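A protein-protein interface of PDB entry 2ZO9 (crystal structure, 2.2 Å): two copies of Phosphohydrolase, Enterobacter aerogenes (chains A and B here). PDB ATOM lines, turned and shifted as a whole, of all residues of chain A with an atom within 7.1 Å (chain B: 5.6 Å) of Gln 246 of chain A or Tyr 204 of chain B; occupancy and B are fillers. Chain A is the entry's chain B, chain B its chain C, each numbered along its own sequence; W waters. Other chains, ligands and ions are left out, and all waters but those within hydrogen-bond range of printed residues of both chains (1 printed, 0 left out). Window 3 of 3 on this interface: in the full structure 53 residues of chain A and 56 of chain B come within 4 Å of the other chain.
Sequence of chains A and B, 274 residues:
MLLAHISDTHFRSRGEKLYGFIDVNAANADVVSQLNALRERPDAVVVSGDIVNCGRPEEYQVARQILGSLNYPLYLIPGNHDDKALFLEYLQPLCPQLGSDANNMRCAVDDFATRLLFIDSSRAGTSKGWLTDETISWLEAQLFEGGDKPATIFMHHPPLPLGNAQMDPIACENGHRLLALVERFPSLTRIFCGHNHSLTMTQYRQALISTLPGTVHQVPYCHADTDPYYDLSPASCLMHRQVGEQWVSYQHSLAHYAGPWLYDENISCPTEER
Water W1 lies within hydrogen-bond range of N of Trp 247 of chain A (2.8 Å), NH1 of Arg 190 of chain A (3.3 Å), OE1 of Gln 246 of chain A (3.4 Å) and O of Gln 203 of chain B (3.5 Å).
Gln 203 of chain B touches Gln 203 of chain A (CB to NE2, 2.9 Å). Gln 203 of chain A touches Arg 205 of chain B (OE1 to O, 3.6 Å). Arg 205 of chain B touches Gln 206 of chain A (O to CA, 3.5 Å). CD of Gln 246 of chain A touches CD1 of Leu 160 of chain B, 3.9 Å away. Gln 246 of chain A touches Tyr 204 of chain B (NE2 to CD1, 3.3 Å).
Of the printed residues of chain B, Arg 190 of chain A touches Gln 203. Arg 241 of chain A touches none of the printed residues of chain B. Of chain B, only Leu 160 (3.9 Å), Thr 202 (3.2 Å), Gln 203 (2.9 Å) and Tyr 204 (3.3 Å) come within 4 Å of Gln 246 of chain A. Of the printed residues of chain A, Leu 160 of chain B touches Gln 246. Pro 161 of chain B touches none of the printed residues of chain A. Printed residues of chain A within 4 Å of Gln 203 of chain B: Arg 190 (2.4 Å), Gln 203 (2.9 Å), Gln 206 (3.0 Å) and Gln 246 (2.9 Å). Tyr 204 of chain B touches one residue of chain A. Printed residues of chain A within 4 Å of Arg 205 of chain B: Gln 203 (3.6 Å) and Gln 206 (3.5 Å). The nearest residue of chain A that does not touch Tyr 204 of chain B is Gln 203 of chain A (4.8 Å).
NH2 of Arg 190 of chain A sits at hydrogen-bond distance from OE1 of Gln 203 of chain B, 2.4 Å away. The backbone carbonyl oxygen (O) of Gln 206 of chain B lies close to the side-chain amide oxygen (OE1) of Gln 203 of chain A, at 3.2 Å. NE2 of Gln 203 of chain A lies within hydrogen-bond range of O of Ala 207 of chain B, at 3.4 Å. NE2 of Gln 203 of chain A sits close to N of Leu 208 of chain B (3.4 Å). The backbone carbonyl oxygen (O) of Gln 206 of chain A sits at hydrogen-bond distance from the side-chain amide nitrogen (NE2) of Gln 203 of chain B (3.0 Å). The side-chain amide oxygen (OE1) of Gln 246 of chain A sits at hydrogen-bond distance from the side-chain hydroxyl (OG1) of Thr 202 of chain B, 3.2 Å away. OE1 of Gln 246 of chain A lies close to O of Gln 203 of chain B (2.9 Å). The backbone carbonyl oxygen (O) of Trp 247 of chain A is in hydrogen-bond range of the side-chain hydroxyl (OG1) of Thr 202 of chain B, at 2.7 Å.
Printed residues of chain B that touch a printed residue of chain A: Leu 160, Thr 202, Gln 203, Tyr 204, Arg 205, Gln 206, Ala 207 and Leu 208. Hydrophobic or aromatic side chains of chain B within 4 Å of the printed part of chain A: Leu 160, Tyr 204 and Leu 208. Of the 12 printed residues of chain A, 5 touch a printed residue of chain B. Printed residues of chain A that touch a printed residue of chain B: Arg 190, Gln 203, Gln 206, Gln 246 and Trp 247. Along chain A the printed residues that touch a printed residue of chain B span positions 190 to 247. Among the printed residues, 13 pairs touch across the chains.
Gln 203 of chain A touches its own counterpart, Gln 203 of chain B. Gln 203 of chain A touches Gln 206 of chain B, and with the chains exchanged Gln 206 of chain A touches Gln 203 of chain B. 2 positions are printed for both chains. Of the 13 pairs that touch across the chains among the printed residues, 3 have their exchanged pair printed and touching as well.
The guanidinium group (NH1) of Arg 190 of chain A is in hydrogen-bond range of the backbone carbonyl oxygen (O) of Trp 247 of chain A. O of Val 182 of chain B sits close to OE1 of Gln 206 of chain B (2.9 Å). The side-chain carboxylate (OE1) of Glu 183 of chain B lies within hydrogen-bond range of the side-chain hydroxyl (OH) of Tyr 204 of chain B (2.5 Å). The side-chain carboxylate (OE1) of Glu 183 of chain B is in salt-bridge range of the guanidinium group (NH1) of Arg 205 of chain B (3.4 Å). O of Thr 202 of chain B is in hydrogen-bond range of N of Ile 209 of chain B. NE2 of Gln 203 of chain B is in hydrogen-bond range of O of Arg 205 of chain B, 2.7 Å away.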
ATOM      1  N   THR A 114     -37.660 -24.097 -23.138  1.00  0.00           N
ATOM      2  CA  THR A 114     -37.304 -23.271 -21.974  1.00  0.00           C
ATOM      3  C   THR A 114     -38.207 -22.024 -21.941  1.00  0.00           C
ATOM      4  O   THR A 114     -38.379 -21.362 -22.964  1.00  0.00           O
ATOM      5  CB  THR A 114     -35.809 -22.864 -22.035  1.00  0.00           C
ATOM      6  OG1 THR A 114     -34.997 -24.041 -22.033  1.00  0.00           O
ATOM      7  CG2 THR A 114     -35.404 -21.996 -20.857  1.00  0.00           C
ATOM      8  N   ARG A 190     -30.787 -19.771 -16.274  1.00  0.00           N
ATOM      9  CA  ARG A 190     -30.076 -18.758 -17.105  1.00  0.00           C
ATOM     10  C   ARG A 190     -30.558 -17.348 -16.721  1.00  0.00           C
ATOM     11  O   ARG A 190     -31.771 -17.108 -16.558  1.00  0.00           O
ATOM     12  CB  ARG A 190     -30.314 -18.899 -18.620  1.00  0.00           C
ATOM     13  CG  ARG A 190     -29.771 -20.069 -19.477  1.00  0.00           C
ATOM     14  CD  ARG A 190     -28.208 -20.270 -19.575  1.00  0.00           C
ATOM     15  NE  ARG A 190     -28.087 -21.342 -18.649  1.00  0.00           N
ATOM     16  CZ  ARG A 190     -27.929 -22.626 -18.904  1.00  0.00           C
ATOM     17  NH1 ARG A 190     -27.617 -23.106 -20.103  1.00  0.00           N
ATOM     18  NH2 ARG A 190     -28.003 -23.414 -17.856  1.00  0.00           N
ATOM     19  N   GLN A 203     -21.555 -18.473 -12.382  1.00  0.00           N
ATOM     20  CA  GLN A 203     -22.666 -19.339 -11.960  1.00  0.00           C
ATOM     21  C   GLN A 203     -22.973 -19.133 -10.503  1.00  0.00           C
ATOM     22  O   GLN A 203     -22.080 -18.985  -9.674  1.00  0.00           O
ATOM     23  CB  GLN A 203     -22.450 -20.867 -12.209  1.00  0.00           C
ATOM     24  CG  GLN A 203     -22.886 -21.290 -13.629  1.00  0.00           C
ATOM     25  CD  GLN A 203     -23.674 -22.617 -13.769  1.00  0.00           C
ATOM     26  OE1 GLN A 203     -24.130 -23.236 -12.798  1.00  0.00           O
ATOM     27  NE2 GLN A 203     -23.839 -23.036 -15.022  1.00  0.00           N
ATOM     28  N   GLN A 206     -27.457 -23.368  -9.713  1.00  0.00           N
ATOM     29  CA  GLN A 206     -27.699 -23.976 -11.020  1.00  0.00           C
ATOM     30  C   GLN A 206     -27.826 -22.921 -12.130  1.00  0.00           C
ATOM     31  O   GLN A 206     -27.943 -23.265 -13.301  1.00  0.00           O
ATOM     32  CB  GLN A 206     -28.950 -24.876 -10.953  1.00  0.00           C
ATOM     33  CG  GLN A 206     -30.285 -24.117 -11.027  1.00  0.00           C
ATOM     34  CD  GLN A 206     -30.672 -23.398  -9.725  1.00  0.00           C
ATOM     35  OE1 GLN A 206     -31.512 -22.504  -9.731  1.00  0.00           O
ATOM     36  NE2 GLN A 206     -30.083 -23.797  -8.616  1.00  0.00           N
ATOM     37  N   ARG A 241     -29.180 -21.397 -28.418  1.00  0.00           N
ATOM     38  CA  ARG A 241     -29.791 -22.541 -29.063  1.00  0.00           C
ATOM     39  C   ARG A 241     -30.146 -23.624 -28.058  1.00  0.00           C
ATOM     40  O   ARG A 241     -29.351 -23.939 -27.168  1.00  0.00           O
ATOM     41  CB  ARG A 241     -28.858 -23.118 -30.134  1.00  0.00           C
ATOM     42  CG  ARG A 241     -29.559 -24.081 -31.054  1.00  0.00           C
ATOM     43  CD  ARG A 241     -28.627 -24.790 -31.982  1.00  0.00           C
ATOM     44  NE  ARG A 241     -28.017 -23.867 -32.930  1.00  0.00           N
ATOM     45  CZ  ARG A 241     -28.522 -23.550 -34.129  1.00  0.00           C
ATOM     46  NH1 ARG A 241     -29.692 -24.090 -34.521  1.00  0.00           N
ATOM     47  NH2 ARG A 241     -27.838 -22.694 -34.928  1.00  0.00           N
ATOM     48  N   GLN A 242     -31.336 -24.197 -28.210  1.00  0.00           N
ATOM     49  CA  GLN A 242     -31.705 -25.357 -27.440  1.00  0.00           C
ATOM     50  C   GLN A 242     -31.203 -26.618 -28.141  1.00  0.00           C
ATOM     51  O   GLN A 242     -31.617 -26.914 -29.263  1.00  0.00           O
ATOM     52  CB  GLN A 242     -33.223 -25.421 -27.244  1.00  0.00           C
ATOM     53  CG  GLN A 242     -33.673 -26.537 -26.340  1.00  0.00           C
ATOM     54  CD  GLN A 242     -33.551 -26.193 -24.858  1.00  0.00           C
ATOM     55  OE1 GLN A 242     -33.142 -27.042 -24.045  1.00  0.00           O
ATOM     56  NE2 GLN A 242     -33.952 -24.965 -24.486  1.00  0.00           N
ATOM     57  N   VAL A 243     -30.317 -27.352 -27.462  1.00  0.00           N
ATOM     58  CA  VAL A 243     -29.676 -28.563 -27.981  1.00  0.00           C
ATOM     59  C   VAL A 243     -30.017 -29.731 -27.044  1.00  0.00           C
ATOM     60  O   VAL A 243     -29.314 -29.966 -26.051  1.00  0.00           O
ATOM     61  CB  VAL A 243     -28.124 -28.357 -28.124  1.00  0.00           C
ATOM     62  CG1 VAL A 243     -27.437 -29.573 -28.728  1.00  0.00           C
ATOM     63  CG2 VAL A 243     -27.824 -27.127 -28.967  1.00  0.00           C
ATOM     64  N   GLY A 244     -31.109 -30.446 -27.347  1.00  0.00           N
ATOM     65  CA  GLY A 244     -31.668 -31.437 -26.424  1.00  0.00           C
ATOM     66  C   GLY A 244     -32.026 -30.760 -25.110  1.00  0.00           C
ATOM     67  O   GLY A 244     -32.742 -29.756 -25.102  1.00  0.00           O
ATOM     68  N   GLU A 245     -31.485 -31.286 -24.008  1.00  0.00           N
ATOM     69  CA  GLU A 245     -31.704 -30.743 -22.654  1.00  0.00           C
ATOM     70  C   GLU A 245     -30.893 -29.481 -22.347  1.00  0.00           C
ATOM     71  O   GLU A 245     -31.102 -28.850 -21.316  1.00  0.00           O
ATOM     72  CB  GLU A 245     -31.330 -31.791 -21.599  1.00  0.00           C
ATOM     73  CG  GLU A 245     -32.496 -32.498 -20.912  1.00  0.00           C
ATOM     74  CD  GLU A 245     -32.117 -33.000 -19.472  1.00  0.00           C
ATOM     75  OE1 GLU A 245     -30.937 -33.454 -19.251  1.00  0.00           O
ATOM     76  OE2 GLU A 245     -33.009 -32.917 -18.569  1.00  0.00           O
ATOM     77  N   GLN A 246     -29.962 -29.145 -23.234  1.00  0.00           N
ATOM     78  CA  GLN A 246     -28.975 -28.099 -23.004  1.00  0.00           C
ATOM     79  C   GLN A 246     -29.329 -26.786 -23.701  1.00  0.00           C
ATOM     80  O   GLN A 246     -29.604 -26.761 -24.897  1.00  0.00           O
ATOM     81  CB  GLN A 246     -27.581 -28.564 -23.454  1.00  0.00           C
ATOM     82  CG  GLN A 246     -27.057 -29.788 -22.680  1.00  0.00           C
ATOM     83  CD  GLN A 246     -26.925 -29.499 -21.188  1.00  0.00           C
ATOM     84  OE1 GLN A 246     -26.425 -28.431 -20.803  1.00  0.00           O
ATOM     85  NE2 GLN A 246     -27.363 -30.437 -20.346  1.00  0.00           N
ATOM     86  N   TRP A 247     -29.328 -25.699 -22.932  1.00  0.00           N
ATOM     87  CA  TRP A 247     -29.352 -24.356 -23.490  1.00  0.00           C
ATOM     88  C   TRP A 247     -27.885 -23.999 -23.746  1.00  0.00           C
ATOM     89  O   TRP A 247     -27.087 -23.941 -22.803  1.00  0.00           O
ATOM     90  CB  TRP A 247     -30.013 -23.390 -22.489  1.00  0.00           C
ATOM     91  CG  TRP A 247     -30.014 -21.927 -22.921  1.00  0.00           C
ATOM     92  CD1 TRP A 247     -28.929 -21.144 -23.135  1.00  0.00           C
ATOM     93  CD2 TRP A 247     -31.165 -21.099 -23.172  1.00  0.00           C
ATOM     94  NE1 TRP A 247     -29.316 -19.892 -23.511  1.00  0.00           N
ATOM     95  CE2 TRP A 247     -30.684 -19.827 -23.536  1.00  0.00           C
ATOM     96  CE3 TRP A 247     -32.553 -21.315 -23.122  1.00  0.00           C
ATOM     97  CZ2 TRP A 247     -31.540 -18.759 -23.844  1.00  0.00           C
ATOM     98  CZ3 TRP A 247     -33.396 -20.273 -23.438  1.00  0.00           C
ATOM     99  CH2 TRP A 247     -32.888 -18.999 -23.796  1.00  0.00           C
ATOM    100  N   VAL A 248     -27.507 -23.826 -25.015  1.00  0.00           N
ATOM    101  CA  VAL A 248     -26.142 -23.407 -25.311  1.00  0.00           C
ATOM    102  C   VAL A 248     -26.122 -21.994 -25.927  1.00  0.00           C
ATOM    103  O   VAL A 248     -26.979 -21.639 -26.749  1.00  0.00           O
ATOM    104  CB  VAL A 248     -25.220 -24.502 -26.021  1.00  0.00           C
ATOM    105  CG1 VAL A 248     -25.850 -25.926 -25.982  1.00  0.00           C
ATOM    106  CG2 VAL A 248     -24.774 -24.105 -27.388  1.00  0.00           C
ATOM    107  N   LEU B 160     -19.444 -32.565 -23.531  1.00  0.00           N
ATOM    108  CA  LEU B 160     -20.799 -32.849 -24.041  1.00  0.00           C
ATOM    109  C   LEU B 160     -20.935 -32.192 -25.397  1.00  0.00           C
ATOM    110  O   LEU B 160     -20.161 -31.276 -25.706  1.00  0.00           O
ATOM    111  CB  LEU B 160     -21.923 -32.381 -23.071  1.00  0.00           C
ATOM    112  CG  LEU B 160     -22.218 -30.885 -22.805  1.00  0.00           C
ATOM    113  CD1 LEU B 160     -23.260 -30.739 -21.725  1.00  0.00           C
ATOM    114  CD2 LEU B 160     -20.975 -30.086 -22.449  1.00  0.00           C
ATOM    115  N   PRO B 161     -21.874 -32.698 -26.230  1.00  0.00           N
ATOM    116  CA  PRO B 161     -22.241 -32.062 -27.505  1.00  0.00           C
ATOM    117  C   PRO B 161     -22.808 -30.671 -27.287  1.00  0.00           C
ATOM    118  O   PRO B 161     -23.633 -30.463 -26.394  1.00  0.00           O
ATOM    119  CB  PRO B 161     -23.324 -32.994 -28.078  1.00  0.00           C
ATOM    120  CG  PRO B 161     -23.813 -33.794 -26.909  1.00  0.00           C
ATOM    121  CD  PRO B 161     -22.613 -33.962 -26.024  1.00  0.00           C
ATOM    122  N   LEU B 179     -19.484 -35.587 -16.845  1.00  0.00           N
ATOM    123  CA  LEU B 179     -20.862 -35.255 -16.449  1.00  0.00           C
ATOM    124  C   LEU B 179     -21.319 -36.048 -15.215  1.00  0.00           C
ATOM    125  O   LEU B 179     -21.983 -35.489 -14.331  1.00  0.00           O
ATOM    126  CB  LEU B 179     -21.819 -35.483 -17.628  1.00  0.00           C
ATOM    127  CG  LEU B 179     -22.207 -34.334 -18.592  1.00  0.00           C
ATOM    128  CD1 LEU B 179     -21.219 -33.154 -18.617  1.00  0.00           C
ATOM    129  CD2 LEU B 179     -22.552 -34.841 -19.995  1.00  0.00           C
ATOM    130  N   VAL B 182     -19.861 -34.363 -12.193  1.00  0.00           N
ATOM    131  CA  VAL B 182     -20.532 -33.138 -11.740  1.00  0.00           C
ATOM    132  C   VAL B 182     -21.812 -33.486 -10.979  1.00  0.00           C
ATOM    133  O   VAL B 182     -22.141 -32.813 -10.004  1.00  0.00           O
ATOM    134  CB  VAL B 182     -20.746 -31.977 -12.826  1.00  0.00           C
ATOM    135  CG1 VAL B 182     -19.806 -32.108 -14.046  1.00  0.00           C
ATOM    136  CG2 VAL B 182     -22.202 -31.778 -13.237  1.00  0.00           C
ATOM    137  N   GLU B 183     -22.510 -34.540 -11.407  1.00  0.00           N
ATOM    138  CA  GLU B 183     -23.640 -35.061 -10.646  1.00  0.00           C
ATOM    139  C   GLU B 183     -23.201 -35.543  -9.260  1.00  0.00           C
ATOM    140  O   GLU B 183     -23.858 -35.248  -8.301  1.00  0.00           O
ATOM    141  CB  GLU B 183     -24.386 -36.164 -11.413  1.00  0.00           C
ATOM    142  CG  GLU B 183     -24.976 -35.680 -12.760  1.00  0.00           C
ATOM    143  CD  GLU B 183     -25.773 -36.769 -13.492  1.00  0.00           C
ATOM    144  OE1 GLU B 183     -26.246 -36.519 -14.622  1.00  0.00           O
ATOM    145  OE2 GLU B 183     -25.918 -37.883 -12.958  1.00  0.00           O
ATOM    146  N   THR B 202     -22.433 -23.344 -21.613  1.00  0.00           N
ATOM    147  CA  THR B 202     -23.607 -24.063 -21.173  1.00  0.00           C
ATOM    148  C   THR B 202     -23.477 -24.385 -19.673  1.00  0.00           C
ATOM    149  O   THR B 202     -22.465 -24.091 -19.040  1.00  0.00           O
ATOM    150  CB  THR B 202     -23.854 -25.329 -22.082  1.00  0.00           C
ATOM    151  OG1 THR B 202     -25.220 -25.730 -21.989  1.00  0.00           O
ATOM    152  CG2 THR B 202     -22.921 -26.510 -21.743  1.00  0.00           C
ATOM    153  N   GLN B 203     -24.514 -24.977 -19.117  1.00  0.00           N
ATOM    154  CA  GLN B 203     -24.594 -25.265 -17.697  1.00  0.00           C
ATOM    155  C   GLN B 203     -25.138 -26.671 -17.575  1.00  0.00           C
ATOM    156  O   GLN B 203     -26.106 -27.029 -18.242  1.00  0.00           O
ATOM    157  CB  GLN B 203     -25.508 -24.237 -17.002  1.00  0.00           C
ATOM    158  CG  GLN B 203     -26.138 -24.621 -15.649  1.00  0.00           C
ATOM    159  CD  GLN B 203     -27.514 -25.450 -15.704  1.00  0.00           C
ATOM    160  OE1 GLN B 203     -28.173 -25.590 -16.763  1.00  0.00           O
ATOM    161  NE2 GLN B 203     -27.930 -25.976 -14.525  1.00  0.00           N
ATOM    162  N   TYR B 204     -24.487 -27.464 -16.737  1.00  0.00           N
ATOM    163  CA  TYR B 204     -24.958 -28.798 -16.403  1.00  0.00           C
ATOM    164  C   TYR B 204     -24.964 -28.876 -14.873  1.00  0.00           C
ATOM    165  O   TYR B 204     -23.899 -28.839 -14.258  1.00  0.00           O
ATOM    166  CB  TYR B 204     -24.045 -29.849 -17.029  1.00  0.00           C
ATOM    167  CG  TYR B 204     -24.616 -31.228 -16.937  1.00  0.00           C
ATOM    168  CD1 TYR B 204     -25.462 -31.718 -17.933  1.00  0.00           C
ATOM    169  CD2 TYR B 204     -24.356 -32.039 -15.827  1.00  0.00           C
ATOM    170  CE1 TYR B 204     -26.024 -33.001 -17.831  1.00  0.00           C
ATOM    171  CE2 TYR B 204     -24.924 -33.303 -15.708  1.00  0.00           C
ATOM    172  CZ  TYR B 204     -25.742 -33.785 -16.722  1.00  0.00           C
ATOM    173  OH  TYR B 204     -26.299 -35.046 -16.616  1.00  0.00           O
ATOM    174  N   ARG B 205     -26.157 -28.962 -14.269  1.00  0.00           N
ATOM    175  CA  ARG B 205     -26.334 -28.804 -12.813  1.00  0.00           C
ATOM    176  C   ARG B 205     -25.646 -27.519 -12.289  1.00  0.00           C
ATOM    177  O   ARG B 205     -25.918 -26.409 -12.763  1.00  0.00           O
ATOM    178  CB  ARG B 205     -25.842 -30.032 -12.042  1.00  0.00           C
ATOM    179  CG  ARG B 205     -26.189 -31.369 -12.693  1.00  0.00           C
ATOM    180  CD  ARG B 205     -27.661 -31.642 -12.643  1.00  0.00           C
ATOM    181  NE  ARG B 205     -27.858 -32.822 -11.844  1.00  0.00           N
ATOM    182  CZ  ARG B 205     -28.243 -33.996 -12.333  1.00  0.00           C
ATOM    183  NH1 ARG B 205     -28.488 -34.130 -13.639  1.00  0.00           N
ATOM    184  NH2 ARG B 205     -28.370 -35.017 -11.522  1.00  0.00           N
ATOM    185  N   GLN B 206     -24.732 -27.687 -11.338  1.00  0.00           N
ATOM    186  CA  GLN B 206     -24.045 -26.571 -10.707  1.00  0.00           C
ATOM    187  C   GLN B 206     -22.807 -26.135 -11.496  1.00  0.00           C
ATOM    188  O   GLN B 206     -22.168 -25.135 -11.136  1.00  0.00           O
ATOM    189  CB  GLN B 206     -23.681 -26.922  -9.249  1.00  0.00           C
ATOM    190  CG  GLN B 206     -22.422 -27.786  -9.063  1.00  0.00           C
ATOM    191  CD  GLN B 206     -22.616 -29.272  -9.403  1.00  0.00           C
ATOM    192  OE1 GLN B 206     -21.652 -29.974  -9.705  1.00  0.00           O
ATOM    193  NE2 GLN B 206     -23.846 -29.739  -9.380  1.00  0.00           N
ATOM    194  N   ALA B 207     -22.475 -26.883 -12.559  1.00  0.00           N
ATOM    195  CA  ALA B 207     -21.304 -26.591 -13.402  1.00  0.00           C
ATOM    196  C   ALA B 207     -21.570 -25.712 -14.648  1.00  0.00           C
ATOM    197  O   ALA B 207     -22.406 -26.044 -15.507  1.00  0.00           O
ATOM    198  CB  ALA B 207     -20.594 -27.882 -13.817  1.00  0.00           C
ATOM    199  N   LEU B 208     -20.840 -24.595 -14.728  1.00  0.00           N
ATOM    200  CA  LEU B 208     -20.665 -23.833 -15.968  1.00  0.00           C
ATOM    201  C   LEU B 208     -19.581 -24.507 -16.810  1.00  0.00           C
ATOM    202  O   LEU B 208     -18.497 -24.837 -16.315  1.00  0.00           O
ATOM    203  CB  LEU B 208     -20.400 -22.340 -15.639  1.00  0.00           C
ATOM    204  CG  LEU B 208     -19.799 -21.175 -16.457  1.00  0.00           C
ATOM    205  CD1 LEU B 208     -19.374 -21.449 -17.901  1.00  0.00           C
ATOM    206  CD2 LEU B 208     -20.624 -19.878 -16.301  1.00  0.00           C
ATOM    207  N   ILE B 209     -19.924 -24.778 -18.067  1.00  0.00           N
ATOM    208  CA  ILE B 209     -19.015 -25.430 -19.013  1.00  0.00           C
ATOM    209  C   ILE B 209     -18.825 -24.502 -20.221  1.00  0.00           C
ATOM    210  O   ILE B 209     -19.790 -24.109 -20.887  1.00  0.00           O
ATOM    211  CB  ILE B 209     -19.524 -26.819 -19.449  1.00  0.00           C
ATOM    212  CG1 ILE B 209     -19.903 -27.658 -18.214  1.00  0.00           C
ATOM    213  CG2 ILE B 209     -18.479 -27.544 -20.348  1.00  0.00           C
ATOM    214  CD1 ILE B 209     -20.510 -29.037 -18.520  1.00  0.00           C
HETATM  215  O   HOH W   1     -28.865 -26.178 -20.190  1.00  0.00           O
